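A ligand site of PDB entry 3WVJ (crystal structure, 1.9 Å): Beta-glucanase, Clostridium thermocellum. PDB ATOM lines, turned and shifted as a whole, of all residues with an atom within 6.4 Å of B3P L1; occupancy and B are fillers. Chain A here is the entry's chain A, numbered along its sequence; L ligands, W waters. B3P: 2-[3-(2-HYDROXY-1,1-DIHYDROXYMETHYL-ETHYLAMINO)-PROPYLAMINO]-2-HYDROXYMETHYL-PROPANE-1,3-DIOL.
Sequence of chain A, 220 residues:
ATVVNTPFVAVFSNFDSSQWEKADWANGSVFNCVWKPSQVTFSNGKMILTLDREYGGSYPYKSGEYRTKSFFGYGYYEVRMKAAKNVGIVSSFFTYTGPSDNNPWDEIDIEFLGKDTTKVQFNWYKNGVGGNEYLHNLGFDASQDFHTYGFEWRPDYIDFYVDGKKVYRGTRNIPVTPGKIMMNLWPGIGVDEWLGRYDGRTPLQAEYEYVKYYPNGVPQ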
ATOM      1  N   ASN A  27      -8.906  17.697  21.443  1.00  0.00           N
ATOM      2  CA  ASN A  27      -8.265  16.809  20.406  1.00  0.00           C
ATOM      3  C   ASN A  27      -9.289  15.853  19.857  1.00  0.00           C
ATOM      4  O   ASN A  27      -9.176  15.493  18.667  1.00  0.00           O
ATOM      5  CB  ASN A  27      -7.110  16.005  21.023  1.00  0.00           C
ATOM      6  CG  ASN A  27      -6.381  15.180  20.003  1.00  0.00           C
ATOM      7  OD1 ASN A  27      -5.783  15.738  19.093  1.00  0.00           O
ATOM      8  ND2 ASN A  27      -6.485  13.824  20.105  1.00  0.00           N
ATOM      9  N   SER A  29     -11.107  12.129  19.472  1.00  0.00           N
ATOM     10  CA  SER A  29     -10.468  10.840  19.497  1.00  0.00           C
ATOM     11  C   SER A  29     -10.581  10.138  20.871  1.00  0.00           C
ATOM     12  O   SER A  29     -11.664  10.163  21.496  1.00  0.00           O
ATOM     13  CB  SER A  29      -8.985  11.027  19.083  1.00  0.00           C
ATOM     14  OG  SER A  29      -8.348   9.736  19.199  1.00  0.00           O
ATOM     15  N   VAL A  30      -9.526   9.509  21.387  1.00  0.00           N
ATOM     16  CA  VAL A  30      -9.726   8.753  22.645  1.00  0.00           C
ATOM     17  C   VAL A  30      -9.464   9.586  23.876  1.00  0.00           C
ATOM     18  O   VAL A  30      -9.290   9.017  24.943  1.00  0.00           O
ATOM     19  CB  VAL A  30      -8.927   7.439  22.680  1.00  0.00           C
ATOM     20  CG1 VAL A  30      -9.458   6.480  21.613  1.00  0.00           C
ATOM     21  CG2 VAL A  30      -7.412   7.669  22.419  1.00  0.00           C
ATOM     22  N   PHE A  31      -9.428  10.900  23.733  1.00  0.00           N
ATOM     23  CA  PHE A  31      -8.954  11.842  24.807  1.00  0.00           C
ATOM     24  C   PHE A  31     -10.222  12.396  25.449  1.00  0.00           C
ATOM     25  O   PHE A  31     -10.990  13.066  24.759  1.00  0.00           O
ATOM     26  CB  PHE A  31      -8.183  13.010  24.163  1.00  0.00           C
ATOM     27  CG  PHE A  31      -6.840  12.653  23.589  1.00  0.00           C
ATOM     28  CD1 PHE A  31      -5.656  13.287  24.051  1.00  0.00           C
ATOM     29  CD2 PHE A  31      -6.711  11.694  22.636  1.00  0.00           C
ATOM     30  CE1 PHE A  31      -4.407  12.966  23.494  1.00  0.00           C
ATOM     31  CE2 PHE A  31      -5.457  11.370  22.062  1.00  0.00           C
ATOM     32  CZ  PHE A  31      -4.302  11.954  22.538  1.00  0.00           C
ATOM     33  N   VAL A  90      -2.508   9.046  30.446  1.00  0.00           N
ATOM     34  CA  VAL A  90      -1.250   9.000  29.713  1.00  0.00           C
ATOM     35  C   VAL A  90      -0.525  10.316  29.922  1.00  0.00           C
ATOM     36  O   VAL A  90      -1.174  11.409  29.821  1.00  0.00           O
ATOM     37  CB  VAL A  90      -1.482   8.852  28.193  1.00  0.00           C
ATOM     38  CG1 VAL A  90      -0.222   9.157  27.365  1.00  0.00           C
ATOM     39  CG2 VAL A  90      -1.965   7.424  27.857  1.00  0.00           C
ATOM     40  N   TRP A 105      -0.407  11.840   8.585  1.00  0.00           N
ATOM     41  CA  TRP A 105      -0.277  11.670  10.016  1.00  0.00           C
ATOM     42  C   TRP A 105       0.901  10.822  10.326  1.00  0.00           C
ATOM     43  O   TRP A 105       0.836   9.585  10.235  1.00  0.00           O
ATOM     44  CB  TRP A 105      -1.549  11.082  10.547  1.00  0.00           C
ATOM     45  CG  TRP A 105      -1.549  10.673  12.000  1.00  0.00           C
ATOM     46  CD1 TRP A 105      -0.582  10.888  12.925  1.00  0.00           C
ATOM     47  CD2 TRP A 105      -2.594   9.995  12.717  1.00  0.00           C
ATOM     48  NE1 TRP A 105      -0.935  10.388  14.120  1.00  0.00           N
ATOM     49  CE2 TRP A 105      -2.127   9.852  14.062  1.00  0.00           C
ATOM     50  CE3 TRP A 105      -3.818   9.502  12.382  1.00  0.00           C
ATOM     51  CZ2 TRP A 105      -2.870   9.228  15.013  1.00  0.00           C
ATOM     52  CZ3 TRP A 105      -4.566   8.898  13.364  1.00  0.00           C
ATOM     53  CH2 TRP A 105      -4.087   8.753  14.652  1.00  0.00           C
ATOM     54  N   GLU A 107       3.977  10.394  13.201  1.00  0.00           N
ATOM     55  CA  GLU A 107       4.044  10.707  14.659  1.00  0.00           C
ATOM     56  C   GLU A 107       4.920   9.681  15.359  1.00  0.00           C
ATOM     57  O   GLU A 107       4.892   8.493  15.025  1.00  0.00           O
ATOM     58  CB  GLU A 107       2.631  10.660  15.265  1.00  0.00           C
ATOM     59  CG  GLU A 107       2.585  10.613  16.851  1.00  0.00           C
ATOM     60  CD  GLU A 107       1.214  10.786  17.416  1.00  0.00           C
ATOM     61  OE1 GLU A 107       0.251  11.012  16.646  1.00  0.00           O
ATOM     62  OE2 GLU A 107       1.043  10.687  18.681  1.00  0.00           O
ATOM     63  N   ASP A 109       5.762   8.444  19.322  1.00  0.00           N
ATOM     64  CA  ASP A 109       5.279   8.657  20.684  1.00  0.00           C
ATOM     65  C   ASP A 109       6.135   7.978  21.727  1.00  0.00           C
ATOM     66  O   ASP A 109       6.588   6.796  21.550  1.00  0.00           O
ATOM     67  CB  ASP A 109       3.936   7.974  20.771  1.00  0.00           C
ATOM     68  CG  ASP A 109       2.907   8.642  19.927  1.00  0.00           C
ATOM     69  OD1 ASP A 109       2.757   9.875  20.030  1.00  0.00           O
ATOM     70  OD2 ASP A 109       2.229   7.919  19.203  1.00  0.00           O
ATOM     71  N   GLU A 111       5.059   7.306  25.589  1.00  0.00           N
ATOM     72  CA  GLU A 111       3.851   7.480  26.373  1.00  0.00           C
ATOM     73  C   GLU A 111       3.938   6.669  27.680  1.00  0.00           C
ATOM     74  O   GLU A 111       4.315   5.454  27.683  1.00  0.00           O
ATOM     75  CB  GLU A 111       2.631   6.992  25.577  1.00  0.00           C
ATOM     76  CG  GLU A 111       2.229   8.025  24.515  1.00  0.00           C
ATOM     77  CD  GLU A 111       1.092   7.539  23.644  1.00  0.00           C
ATOM     78  OE1 GLU A 111       1.209   6.492  23.001  1.00  0.00           O
ATOM     79  OE2 GLU A 111       0.053   8.188  23.595  1.00  0.00           O
ATOM     80  N   GLN A 121       5.840   3.205  27.082  1.00  0.00           N
ATOM     81  CA  GLN A 121       5.358   2.676  25.809  1.00  0.00           C
ATOM     82  C   GLN A 121       5.903   3.462  24.612  1.00  0.00           C
ATOM     83  O   GLN A 121       5.863   4.719  24.575  1.00  0.00           O
ATOM     84  CB  GLN A 121       3.843   2.560  25.771  1.00  0.00           C
ATOM     85  CG  GLN A 121       3.405   1.808  24.538  1.00  0.00           C
ATOM     86  CD  GLN A 121       1.929   1.921  24.255  1.00  0.00           C
ATOM     87  OE1 GLN A 121       1.120   1.130  24.764  1.00  0.00           O
ATOM     88  NE2 GLN A 121       1.562   2.913  23.447  1.00  0.00           N
ATOM     89  N   ASN A 123       5.542   4.003  20.383  1.00  0.00           N
ATOM     90  CA  ASN A 123       4.642   3.787  19.276  1.00  0.00           C
ATOM     91  C   ASN A 123       5.010   4.816  18.206  1.00  0.00           C
ATOM     92  O   ASN A 123       5.713   5.795  18.471  1.00  0.00           O
ATOM     93  CB  ASN A 123       3.158   3.921  19.702  1.00  0.00           C
ATOM     94  CG  ASN A 123       2.183   3.351  18.671  1.00  0.00           C
ATOM     95  OD1 ASN A 123       2.543   2.420  17.859  1.00  0.00           O
ATOM     96  ND2 ASN A 123       0.905   3.830  18.718  1.00  0.00           N
ATOM     97  N   TYR A 125       3.349   6.472  14.179  1.00  0.00           N
ATOM     98  CA  TYR A 125       2.404   6.375  13.074  1.00  0.00           C
ATOM     99  C   TYR A 125       3.057   6.777  11.783  1.00  0.00           C
ATOM    100  O   TYR A 125       3.824   7.713  11.764  1.00  0.00           O
ATOM    101  CB  TYR A 125       1.242   7.335  13.257  1.00  0.00           C
ATOM    102  CG  TYR A 125       0.323   6.874  14.331  1.00  0.00           C
ATOM    103  CD1 TYR A 125      -0.854   6.243  14.017  1.00  0.00           C
ATOM    104  CD2 TYR A 125       0.642   7.077  15.689  1.00  0.00           C
ATOM    105  CE1 TYR A 125      -1.692   5.806  15.022  1.00  0.00           C
ATOM    106  CE2 TYR A 125      -0.201   6.644  16.711  1.00  0.00           C
ATOM    107  CZ  TYR A 125      -1.371   5.989  16.335  1.00  0.00           C
ATOM    108  OH  TYR A 125      -2.263   5.529  17.301  1.00  0.00           O
ATOM    109  N   GLU A 133       2.924  -0.394  19.135  1.00  0.00           N
ATOM    110  CA  GLU A 133       3.006  -0.287  20.599  1.00  0.00           C
ATOM    111  C   GLU A 133       4.019  -1.289  21.142  1.00  0.00           C
ATOM    112  O   GLU A 133       3.841  -2.495  20.985  1.00  0.00           O
ATOM    113  CB  GLU A 133       1.603  -0.507  21.173  1.00  0.00           C
ATOM    114  CG  GLU A 133       0.633   0.657  20.884  1.00  0.00           C
ATOM    115  CD  GLU A 133      -0.202   0.467  19.631  1.00  0.00           C
ATOM    116  OE1 GLU A 133       0.116  -0.456  18.818  1.00  0.00           O
ATOM    117  OE2 GLU A 133      -1.198   1.247  19.424  1.00  0.00           O
ATOM    118  N   TRP A 186      -3.406  13.218  29.534  1.00  0.00           N
ATOM    119  CA  TRP A 186      -4.827  13.070  29.351  1.00  0.00           C
ATOM    120  C   TRP A 186      -5.423  11.848  29.911  1.00  0.00           C
ATOM    121  O   TRP A 186      -4.747  10.836  29.998  1.00  0.00           O
ATOM    122  CB  TRP A 186      -5.140  13.168  27.855  1.00  0.00           C
ATOM    123  CG  TRP A 186      -4.245  12.314  26.987  1.00  0.00           C
ATOM    124  CD1 TRP A 186      -2.933  12.590  26.579  1.00  0.00           C
ATOM    125  CD2 TRP A 186      -4.616  10.990  26.394  1.00  0.00           C
ATOM    126  NE1 TRP A 186      -2.476  11.599  25.742  1.00  0.00           N
ATOM    127  CE2 TRP A 186      -3.432  10.549  25.648  1.00  0.00           C
ATOM    128  CE3 TRP A 186      -5.727  10.163  26.472  1.00  0.00           C
ATOM    129  CZ2 TRP A 186      -3.412   9.352  24.928  1.00  0.00           C
ATOM    130  CZ3 TRP A 186      -5.704   8.932  25.723  1.00  0.00           C
ATOM    131  CH2 TRP A 186      -4.572   8.553  24.970  1.00  0.00           C
ATOM    132  N   GLY A 190     -12.751   4.982  26.069  1.00  0.00           N
ATOM    133  CA  GLY A 190     -12.970   3.942  25.051  1.00  0.00           C
ATOM    134  C   GLY A 190     -11.748   3.063  24.917  1.00  0.00           C
ATOM    135  O   GLY A 190     -11.609   2.333  23.949  1.00  0.00           O
ATOM    136  N   VAL A 191     -10.822   3.173  25.863  1.00  0.00           N
ATOM    137  CA  VAL A 191      -9.573   2.452  25.756  1.00  0.00           C
ATOM    138  C   VAL A 191      -9.187   1.787  27.097  1.00  0.00           C
ATOM    139  O   VAL A 191      -8.011   1.812  27.512  1.00  0.00           O
ATOM    140  CB  VAL A 191      -8.415   3.333  25.213  1.00  0.00           C
ATOM    141  CG1 VAL A 191      -8.584   3.577  23.679  1.00  0.00           C
ATOM    142  CG2 VAL A 191      -8.179   4.607  26.046  1.00  0.00           C
ATOM    143  N   GLU A 193      -8.997  -1.427  28.118  1.00  0.00           N
ATOM    144  CA  GLU A 193      -8.043  -2.547  28.049  1.00  0.00           C
ATOM    145  C   GLU A 193      -6.631  -2.005  27.951  1.00  0.00           C
ATOM    146  O   GLU A 193      -5.695  -2.613  28.487  1.00  0.00           O
ATOM    147  CB  GLU A 193      -8.264  -3.532  26.893  1.00  0.00           C
ATOM    148  CG  GLU A 193      -9.480  -3.292  25.982  1.00  0.00           C
ATOM    149  CD  GLU A 193      -9.662  -1.840  25.429  1.00  0.00           C
ATOM    150  OE1 GLU A 193      -8.706  -1.177  24.842  1.00  0.00           O
ATOM    151  OE2 GLU A 193     -10.824  -1.367  25.562  1.00  0.00           O
ATOM    152  N   TRP A 194      -6.454  -0.855  27.276  1.00  0.00           N
ATOM    153  CA  TRP A 194      -5.131  -0.330  27.122  1.00  0.00           C
ATOM    154  C   TRP A 194      -4.620   0.446  28.326  1.00  0.00           C
ATOM    155  O   TRP A 194      -3.456   0.266  28.764  1.00  0.00           O
ATOM    156  CB  TRP A 194      -5.065   0.488  25.841  1.00  0.00           C
ATOM    157  CG  TRP A 194      -3.762   1.214  25.638  1.00  0.00           C
ATOM    158  CD1 TRP A 194      -2.476   0.719  25.814  1.00  0.00           C
ATOM    159  CD2 TRP A 194      -3.606   2.620  25.213  1.00  0.00           C
ATOM    160  NE1 TRP A 194      -1.551   1.697  25.532  1.00  0.00           N
ATOM    161  CE2 TRP A 194      -2.176   2.856  25.140  1.00  0.00           C
ATOM    162  CE3 TRP A 194      -4.490   3.649  24.862  1.00  0.00           C
ATOM    163  CZ2 TRP A 194      -1.667   4.093  24.724  1.00  0.00           C
ATOM    164  CZ3 TRP A 194      -3.971   4.877  24.450  1.00  0.00           C
ATOM    165  CH2 TRP A 194      -2.608   5.106  24.379  1.00  0.00           C
HETATM  166  C1  B3P L   1      -2.568   4.128  20.379  1.00  0.00           C
HETATM  167  C2  B3P L   1      -3.150   5.532  20.712  1.00  0.00           C
HETATM  168  C3  B3P L   1      -3.291   3.123  21.290  1.00  0.00           C
HETATM  169  N1  B3P L   1      -3.805   2.028  20.435  1.00  0.00           N
HETATM  170  C4  B3P L   1      -4.527   0.943  21.064  1.00  0.00           C
HETATM  171  C5  B3P L   1      -4.660  -0.095  19.917  1.00  0.00           C
HETATM  172  C6  B3P L   1      -3.823   0.420  22.275  1.00  0.00           C
HETATM  173  C7  B3P L   1      -5.892   1.184  21.660  1.00  0.00           C
HETATM  174  N2  B3P L   1      -2.341   6.535  19.988  1.00  0.00           N
HETATM  175  C8  B3P L   1      -3.017   7.878  20.095  1.00  0.00           C
HETATM  176  C9  B3P L   1      -2.342   8.893  19.132  1.00  0.00           C
HETATM  177  C10 B3P L   1      -2.748   8.462  21.495  1.00  0.00           C
HETATM  178  C11 B3P L   1      -4.499   7.827  19.883  1.00  0.00           C
HETATM  179  O1  B3P L   1      -2.998  10.144  19.116  1.00  0.00           O
HETATM  180  O2  B3P L   1      -1.319   8.524  21.485  1.00  0.00           O
HETATM  181  O3  B3P L   1      -4.873   7.153  18.683  1.00  0.00           O
HETATM  182  O4  B3P L   1      -4.875  -1.320  20.572  1.00  0.00           O
HETATM  183  O5  B3P L   1      -2.452   0.171  22.016  1.00  0.00           O
HETATM  184  O6  B3P L   1      -6.429   2.303  21.051  1.00  0.00           O
HETATM  185  C1  B3P L   2      -4.511  15.591  15.919  1.00  0.00           C
HETATM  186  C2  B3P L   2      -4.895  14.209  15.146  1.00  0.00           C
HETATM  187  C3  B3P L   2      -3.200  15.346  16.669  1.00  0.00           C
HETATM  188  N1  B3P L   2      -3.477  14.653  18.004  1.00  0.00           N
HETATM  189  C4  B3P L   2      -2.289  14.446  18.841  1.00  0.00           C
HETATM  190  C5  B3P L   2      -2.917  13.785  20.144  1.00  0.00           C
HETATM  191  C6  B3P L   2      -1.184  13.525  18.247  1.00  0.00           C
HETATM  192  C7  B3P L   2      -1.588  15.869  19.212  1.00  0.00           C
HETATM  193  N2  B3P L   2      -6.224  14.272  14.480  1.00  0.00           N
HETATM  194  C8  B3P L   2      -6.571  12.946  13.803  1.00  0.00           C
HETATM  195  C9  B3P L   2      -7.762  12.964  12.909  1.00  0.00           C
HETATM  196  C10 B3P L   2      -6.773  11.820  14.795  1.00  0.00           C
HETATM  197  C11 B3P L   2      -5.442  12.507  12.866  1.00  0.00           C
HETATM  198  O1  B3P L   2      -8.541  14.047  13.255  1.00  0.00           O
HETATM  199  O2  B3P L   2      -7.234  12.396  16.016  1.00  0.00           O
HETATM  200  O3  B3P L   2      -5.447  13.467  11.837  1.00  0.00           O
HETATM  201  O4  B3P L   2      -1.861  13.537  21.069  1.00  0.00           O
HETATM  202  O5  B3P L   2      -1.871  12.333  17.717  1.00  0.00           O
HETATM  203  O6  B3P L   2      -2.783  16.607  19.712  1.00  0.00           O
HETATM  204  O   HOH W   1      -4.847   4.994  16.506  1.00  0.00           O
HETATM  205  O   HOH W   2       0.334   6.090  20.388  1.00  0.00           O
HETATM  206  O   HOH W   3      -5.227  12.297  18.117  1.00  0.00           O
HETATM  207  O   HOH W   4      -0.509  11.330  20.846  1.00  0.00           O
HETATM  208  O   HOH W   5      -9.333   3.474  19.528  1.00  0.00           O
HETATM  209  O   HOH W   6      -4.457   2.794  17.701  1.00  0.00           O
HETATM  210  O   HOH W   7      -6.531   4.725  19.957  1.00  0.00           O
HETATM  211  O   HOH W   8      -6.202   9.456  17.658  1.00  0.00           O
HETATM  212  O   HOH W   9      -6.323  -2.132  23.537  1.00  0.00           O
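OE2 of Glu 111 sits at hydrogen-bond distance from O2 of B3P L1 (2.5 Å). The side-chain hydroxyl (OH) of Tyr 125 is in hydrogen-bond range of a nitrogen (N2) of B3P L1 (2.9 Å). OE2 of Glu 133 lies within salt-bridge range of N1 of B3P L1 (2.9 Å). An oxygen (O5) of B3P L2 lies within hydrogen-bond range of the side-chain carboxylate (OE1) of Glu 107 (2.7 Å). A nitrogen (N1) of B3P L2 sits at hydrogen-bond distance from the side-chain amide oxygen (OD1) of Asn 27.
An oxygen (O5) of B3P L2 is in hydrogen-bond range of an oxygen (O1) of B3P L1 (2.8 Å).
The backbone carbonyl oxygen (O) of Glu 111 is in hydrogen-bond range of the backbone NH (N) of Gln 121, 2.8 Å away. The backbone carbonyl oxygen (O) of Glu 107 lies within hydrogen-bond range of the backbone NH (N) of Tyr 125 (2.7 Å). N of Glu 133 lies within hydrogen-bond range of OD1 of Asn 123 (3.1 Å). The side-chain amide oxygen (OE1) of Gln 121 sits at hydrogen-bond distance from the indole nitrogen (NE1) of Trp 194 (2.8 Å). The backbone carbonyl oxygen of Val 90 lies within hydrogen-bond range of the backbone NH of Trp 186 (2.9 Å). The indole nitrogen (NE1) of Trp 105 lies within hydrogen-bond range of the side-chain carboxylate (OE1) of Glu 107 (2.9 Å). O of Asn 123 lies within hydrogen-bond range of N of Asp 109 (2.8 Å).
Residues that only touch B3P L1: Val 30, Phe 31, Glu 107, Asn 123, Trp 186, Val 191 and Trp 194.
Water W2 lies within hydrogen-bond range of a nitrogen (N2) of B3P L1 (2.7 Å), the side-chain carboxylate of Glu 111 (2.8 Å), the side-chain amide nitrogen of Asn 123 (2.9 Å) and the side-chain carboxylate of Asp 109 (2.9 Å). Water W8 bridges OG of Ser 29 and O3 of B3P L1. Water W4 lies within hydrogen-bond range of an oxygen (O4) of B3P L2, the side-chain carboxylate (OE2) of Glu 107 and an oxygen (O2) of B3P L1. Water W1 lies within hydrogen-bond range of the side-chain hydroxyl (OH) of Tyr 125 (2.8 Å) and an oxygen (O3) of B3P L1 (3.1 Å). Water W3 lies within hydrogen-bond range of ND2 of Asn 27 (2.8 Å), O2 of B3P L2 (2.9 Å) and O1 of B3P L1 (3.3 Å). Water W9 lies within hydrogen-bond range of the side-chain carboxylate (OE1) of Glu 193 (2.9 Å) and an oxygen (O4) of B3P L1 (3.4 Å).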
